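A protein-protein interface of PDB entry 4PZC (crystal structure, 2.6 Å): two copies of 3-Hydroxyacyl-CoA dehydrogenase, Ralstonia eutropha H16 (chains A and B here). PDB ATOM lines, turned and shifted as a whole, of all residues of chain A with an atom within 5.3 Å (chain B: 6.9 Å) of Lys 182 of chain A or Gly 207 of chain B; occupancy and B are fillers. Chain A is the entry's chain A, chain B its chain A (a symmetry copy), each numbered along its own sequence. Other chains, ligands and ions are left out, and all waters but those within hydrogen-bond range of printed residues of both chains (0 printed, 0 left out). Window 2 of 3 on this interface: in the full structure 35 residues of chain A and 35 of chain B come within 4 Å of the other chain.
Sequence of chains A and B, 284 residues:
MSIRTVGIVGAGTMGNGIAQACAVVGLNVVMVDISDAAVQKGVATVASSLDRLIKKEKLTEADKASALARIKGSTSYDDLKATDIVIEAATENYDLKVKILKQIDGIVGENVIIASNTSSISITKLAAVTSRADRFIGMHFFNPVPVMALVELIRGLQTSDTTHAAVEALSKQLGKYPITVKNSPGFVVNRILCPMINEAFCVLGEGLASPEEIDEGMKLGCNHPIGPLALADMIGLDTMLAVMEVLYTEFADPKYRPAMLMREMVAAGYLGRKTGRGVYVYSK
NZ of Lys 182 of chain A is in hydrogen-bond range of O of Gly 207 of chain B, at 2.6 Å. O of Leu 208 of chain B sits at hydrogen-bond distance from N of Lys 182 of chain A, 2.9 Å away.
Of the 8 printed residues of chain A, 4 touch a printed residue of chain B. Along chain A the printed residues that touch a printed residue of chain B span positions 180 to 184. Of the 10 printed residues of chain B, 3 touch a printed residue of chain A. Hydrophobic or aromatic side chains of chain B within 4 Å of the printed part of chain A: Leu 208 and Ala 209. Among the printed residues, 6 pairs touch across the chains. Among the printed residues, no Asp or Glu carboxylate lies within 4 Å of a Lys or Arg side-chain nitrogen of the other chain.
No position is printed for both chains.
Among the printed residues, pairs that only touch across the chains: Thr 180 of chain A with Leu 208 of chain B (3.8 Å), Thr 180 of chain A with Ala 209 of chain B (3.4 Å), Val 181 of chain A with Leu 208 of chain B (3.3 Å) and Ser 184 of chain A with Leu 208 of chain B (3.7 Å).
Lys 182 of chain A touches two residues of chain B. Printed residues of chain A within 4 Å of Gly 207 of chain B: Lys 182. Printed residues of chain A within 4 Å of Leu 208 of chain B: Thr 180, Val 181, Lys 182 and Ser 184. Printed residues of chain B within 4 Å of Val 181 of chain A: Leu 208. Phe 187 of chain A touches none of the printed residues of chain B. Asn 183 of chain A touches none of the printed residues of chain B. The nearest residue of chain B that does not touch Lys 182 of chain A is Glu 206 of chain B (4.8 Å). The nearest printed residue of chain A that does not touch Gly 207 of chain B is Val 181 of chain A (6.7 Å).
The backbone carbonyl oxygen (O) of Val 203 of chain B lies within hydrogen-bond range of the backbone NH (N) of Leu 208 of chain B (3.3 Å). The backbone NH (N) of Arg 155 of chain A lies within hydrogen-bond range of the backbone carbonyl oxygen (O) of Val 181 of chain A (2.9 Å).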
ATOM      1  N   ILE A 154      -9.928 -12.854   8.082  1.00  0.00           N
ATOM      2  CA  ILE A 154     -10.741 -11.704   7.818  1.00  0.00           C
ATOM      3  C   ILE A 154     -10.365 -10.563   8.746  1.00  0.00           C
ATOM      4  O   ILE A 154     -10.499 -10.642   9.976  1.00  0.00           O
ATOM      5  CB  ILE A 154     -12.214 -12.005   7.946  1.00  0.00           C
ATOM      6  CG1 ILE A 154     -12.562 -13.277   7.171  1.00  0.00           C
ATOM      7  CG2 ILE A 154     -12.999 -10.809   7.436  1.00  0.00           C
ATOM      8  CD1 ILE A 154     -12.980 -14.467   8.024  1.00  0.00           C
ATOM      9  N   ARG A 155      -9.874  -9.498   8.141  1.00  0.00           N
ATOM     10  CA  ARG A 155      -9.390  -8.402   8.909  1.00  0.00           C
ATOM     11  C   ARG A 155     -10.556  -7.530   9.161  1.00  0.00           C
ATOM     12  O   ARG A 155     -11.247  -7.109   8.234  1.00  0.00           O
ATOM     13  CB  ARG A 155      -8.313  -7.654   8.147  1.00  0.00           C
ATOM     14  CG  ARG A 155      -7.029  -8.435   8.136  1.00  0.00           C
ATOM     15  CD  ARG A 155      -5.885  -7.726   7.434  1.00  0.00           C
ATOM     16  NE  ARG A 155      -5.409  -6.533   8.143  1.00  0.00           N
ATOM     17  CZ  ARG A 155      -4.155  -6.090   8.094  1.00  0.00           C
ATOM     18  NH1 ARG A 155      -3.222  -6.759   7.409  1.00  0.00           N
ATOM     19  NH2 ARG A 155      -3.816  -4.988   8.756  1.00  0.00           N
ATOM     20  N   THR A 180      -6.641 -13.942   2.868  1.00  0.00           N
ATOM     21  CA  THR A 180      -6.852 -12.661   3.529  1.00  0.00           C
ATOM     22  C   THR A 180      -7.935 -11.855   2.820  1.00  0.00           C
ATOM     23  O   THR A 180      -8.016 -11.812   1.585  1.00  0.00           O
ATOM     24  CB  THR A 180      -5.533 -11.905   3.680  1.00  0.00           C
ATOM     25  OG1 THR A 180      -4.695 -12.674   4.546  1.00  0.00           O
ATOM     26  CG2 THR A 180      -5.732 -10.539   4.293  1.00  0.00           C
ATOM     27  N   VAL A 181      -8.795 -11.251   3.632  1.00  0.00           N
ATOM     28  CA  VAL A 181     -10.049 -10.708   3.162  1.00  0.00           C
ATOM     29  C   VAL A 181     -10.367  -9.525   4.030  1.00  0.00           C
ATOM     30  O   VAL A 181     -10.379  -9.659   5.243  1.00  0.00           O
ATOM     31  CB  VAL A 181     -11.181 -11.728   3.361  1.00  0.00           C
ATOM     32  CG1 VAL A 181     -12.538 -11.142   3.006  1.00  0.00           C
ATOM     33  CG2 VAL A 181     -10.918 -12.975   2.543  1.00  0.00           C
ATOM     34  N   LYS A 182     -10.609  -8.366   3.425  1.00  0.00           N
ATOM     35  CA  LYS A 182     -11.144  -7.271   4.193  1.00  0.00           C
ATOM     36  C   LYS A 182     -12.559  -7.671   4.577  1.00  0.00           C
ATOM     37  O   LYS A 182     -13.328  -8.056   3.740  1.00  0.00           O
ATOM     38  CB  LYS A 182     -11.189  -5.978   3.392  1.00  0.00           C
ATOM     39  CG  LYS A 182      -9.846  -5.456   2.941  1.00  0.00           C
ATOM     40  CD  LYS A 182     -10.013  -4.002   2.511  1.00  0.00           C
ATOM     41  CE  LYS A 182      -8.699  -3.371   2.049  1.00  0.00           C
ATOM     42  NZ  LYS A 182      -8.323  -3.673   0.629  1.00  0.00           N
ATOM     43  N   ASN A 183     -12.891  -7.568   5.849  1.00  0.00           N
ATOM     44  CA  ASN A 183     -14.248  -7.750   6.305  1.00  0.00           C
ATOM     45  C   ASN A 183     -15.300  -7.129   5.375  1.00  0.00           C
ATOM     46  O   ASN A 183     -15.262  -5.910   5.088  1.00  0.00           O
ATOM     47  CB  ASN A 183     -14.414  -7.159   7.698  1.00  0.00           C
ATOM     48  CG  ASN A 183     -15.722  -7.550   8.323  1.00  0.00           C
ATOM     49  OD1 ASN A 183     -16.030  -8.743   8.439  1.00  0.00           O
ATOM     50  ND2 ASN A 183     -16.527  -6.548   8.707  1.00  0.00           N
ATOM     51  N   SER A 184     -16.236  -7.989   4.943  1.00  0.00           N
ATOM     52  CA  SER A 184     -17.312  -7.647   4.009  1.00  0.00           C
ATOM     53  C   SER A 184     -18.321  -8.803   3.984  1.00  0.00           C
ATOM     54  O   SER A 184     -17.955  -9.982   4.148  1.00  0.00           O
ATOM     55  CB  SER A 184     -16.759  -7.418   2.595  1.00  0.00           C
ATOM     56  OG  SER A 184     -17.762  -7.310   1.583  1.00  0.00           O
ATOM     57  N   PHE A 187     -17.533 -12.341   2.905  1.00  0.00           N
ATOM     58  CA  PHE A 187     -16.106 -12.463   2.691  1.00  0.00           C
ATOM     59  C   PHE A 187     -15.863 -12.846   1.238  1.00  0.00           C
ATOM     60  O   PHE A 187     -16.360 -12.172   0.348  1.00  0.00           O
ATOM     61  CB  PHE A 187     -15.516 -13.444   3.707  1.00  0.00           C
ATOM     62  CG  PHE A 187     -16.031 -13.212   5.105  1.00  0.00           C
ATOM     63  CD1 PHE A 187     -16.235 -11.913   5.573  1.00  0.00           C
ATOM     64  CD2 PHE A 187     -16.350 -14.284   5.940  1.00  0.00           C
ATOM     65  CE1 PHE A 187     -16.743 -11.689   6.837  1.00  0.00           C
ATOM     66  CE2 PHE A 187     -16.862 -14.064   7.210  1.00  0.00           C
ATOM     67  CZ  PHE A 187     -17.059 -12.771   7.657  1.00  0.00           C
ATOM     68  N   PHE B 201     -15.104 -10.670 -10.105  1.00  0.00           N
ATOM     69  CA  PHE B 201     -14.491  -9.403 -10.518  1.00  0.00           C
ATOM     70  C   PHE B 201     -14.890  -8.308  -9.538  1.00  0.00           C
ATOM     71  O   PHE B 201     -14.048  -7.461  -9.175  1.00  0.00           O
ATOM     72  CB  PHE B 201     -14.799  -9.030 -11.972  1.00  0.00           C
ATOM     73  CG  PHE B 201     -13.887  -9.683 -12.942  1.00  0.00           C
ATOM     74  CD1 PHE B 201     -14.030 -11.027 -13.259  1.00  0.00           C
ATOM     75  CD2 PHE B 201     -12.837  -8.986 -13.501  1.00  0.00           C
ATOM     76  CE1 PHE B 201     -13.164 -11.656 -14.158  1.00  0.00           C
ATOM     77  CE2 PHE B 201     -11.954  -9.599 -14.388  1.00  0.00           C
ATOM     78  CZ  PHE B 201     -12.126 -10.929 -14.725  1.00  0.00           C
ATOM     79  N   CYS B 202     -16.141  -8.336  -9.073  1.00  0.00           N
ATOM     80  CA  CYS B 202     -16.571  -7.352  -8.085  1.00  0.00           C
ATOM     81  C   CYS B 202     -15.733  -7.400  -6.819  1.00  0.00           C
ATOM     82  O   CYS B 202     -15.268  -6.366  -6.332  1.00  0.00           O
ATOM     83  CB  CYS B 202     -18.042  -7.532  -7.734  1.00  0.00           C
ATOM     84  SG  CYS B 202     -19.124  -7.412  -9.176  1.00  0.00           S
ATOM     85  N   VAL B 203     -15.544  -8.605  -6.291  1.00  0.00           N
ATOM     86  CA  VAL B 203     -14.775  -8.805  -5.071  1.00  0.00           C
ATOM     87  C   VAL B 203     -13.386  -8.244  -5.288  1.00  0.00           C
ATOM     88  O   VAL B 203     -12.900  -7.458  -4.485  1.00  0.00           O
ATOM     89  CB  VAL B 203     -14.700 -10.305  -4.685  1.00  0.00           C
ATOM     90  CG1 VAL B 203     -13.592 -10.554  -3.692  1.00  0.00           C
ATOM     91  CG2 VAL B 203     -16.022 -10.784  -4.105  1.00  0.00           C
ATOM     92  N   LEU B 204     -12.763  -8.640  -6.390  1.00  0.00           N
ATOM     93  CA  LEU B 204     -11.426  -8.166  -6.735  1.00  0.00           C
ATOM     94  C   LEU B 204     -11.475  -6.658  -6.907  1.00  0.00           C
ATOM     95  O   LEU B 204     -10.674  -5.920  -6.355  1.00  0.00           O
ATOM     96  CB  LEU B 204     -10.953  -8.810  -8.038  1.00  0.00           C
ATOM     97  CG  LEU B 204      -9.664  -8.225  -8.624  1.00  0.00           C
ATOM     98  CD1 LEU B 204      -8.536  -8.465  -7.654  1.00  0.00           C
ATOM     99  CD2 LEU B 204      -9.320  -8.848  -9.959  1.00  0.00           C
ATOM    100  N   GLY B 205     -12.456  -6.209  -7.664  1.00  0.00           N
ATOM    101  CA  GLY B 205     -12.653  -4.791  -7.879  1.00  0.00           C
ATOM    102  C   GLY B 205     -12.711  -3.964  -6.618  1.00  0.00           C
ATOM    103  O   GLY B 205     -12.249  -2.833  -6.611  1.00  0.00           O
ATOM    104  N   GLU B 206     -13.288  -4.514  -5.550  1.00  0.00           N
ATOM    105  CA  GLU B 206     -13.462  -3.753  -4.296  1.00  0.00           C
ATOM    106  C   GLU B 206     -12.227  -3.931  -3.413  1.00  0.00           C
ATOM    107  O   GLU B 206     -12.246  -3.583  -2.213  1.00  0.00           O
ATOM    108  CB  GLU B 206     -14.698  -4.238  -3.538  1.00  0.00           C
ATOM    109  CG  GLU B 206     -16.013  -4.083  -4.300  1.00  0.00           C
ATOM    110  CD  GLU B 206     -17.053  -5.177  -4.011  1.00  0.00           C
ATOM    111  OE1 GLU B 206     -16.924  -5.933  -3.007  1.00  0.00           O
ATOM    112  OE2 GLU B 206     -18.015  -5.273  -4.810  1.00  0.00           O
ATOM    113  N   GLY B 207     -11.173  -4.491  -4.020  1.00  0.00           N
ATOM    114  CA  GLY B 207      -9.948  -4.862  -3.323  1.00  0.00           C
ATOM    115  C   GLY B 207     -10.105  -5.621  -2.023  1.00  0.00           C
ATOM    116  O   GLY B 207      -9.425  -5.329  -1.074  1.00  0.00           O
ATOM    117  N   LEU B 208     -10.992  -6.594  -1.967  1.00  0.00           N
ATOM    118  CA  LEU B 208     -11.224  -7.296  -0.710  1.00  0.00           C
ATOM    119  C   LEU B 208     -10.173  -8.327  -0.519  1.00  0.00           C
ATOM    120  O   LEU B 208      -9.827  -8.664   0.622  1.00  0.00           O
ATOM    121  CB  LEU B 208     -12.578  -8.005  -0.692  1.00  0.00           C
ATOM    122  CG  LEU B 208     -13.744  -7.042  -0.880  1.00  0.00           C
ATOM    123  CD1 LEU B 208     -15.027  -7.841  -0.854  1.00  0.00           C
ATOM    124  CD2 LEU B 208     -13.743  -5.956   0.182  1.00  0.00           C
ATOM    125  N   ALA B 209      -9.689  -8.835  -1.644  1.00  0.00           N
ATOM    126  CA  ALA B 209      -8.700  -9.874  -1.657  1.00  0.00           C
ATOM    127  C   ALA B 209      -7.908  -9.815  -2.953  1.00  0.00           C
ATOM    128  O   ALA B 209      -8.271  -9.107  -3.910  1.00  0.00           O
ATOM    129  CB  ALA B 209      -9.372 -11.221  -1.517  1.00  0.00           C
ATOM    130  N   SER B 210      -6.812 -10.560  -2.971  1.00  0.00           N
ATOM    131  CA  SER B 210      -6.004 -10.662  -4.167  1.00  0.00           C
ATOM    132  C   SER B 210      -6.626 -11.724  -5.075  1.00  0.00           C
ATOM    133  O   SER B 210      -7.314 -12.653  -4.609  1.00  0.00           O
ATOM    134  CB  SER B 210      -4.540 -10.989  -3.852  1.00  0.00           C
ATOM    135  OG  SER B 210      -4.349 -12.389  -3.722  1.00  0.00           O
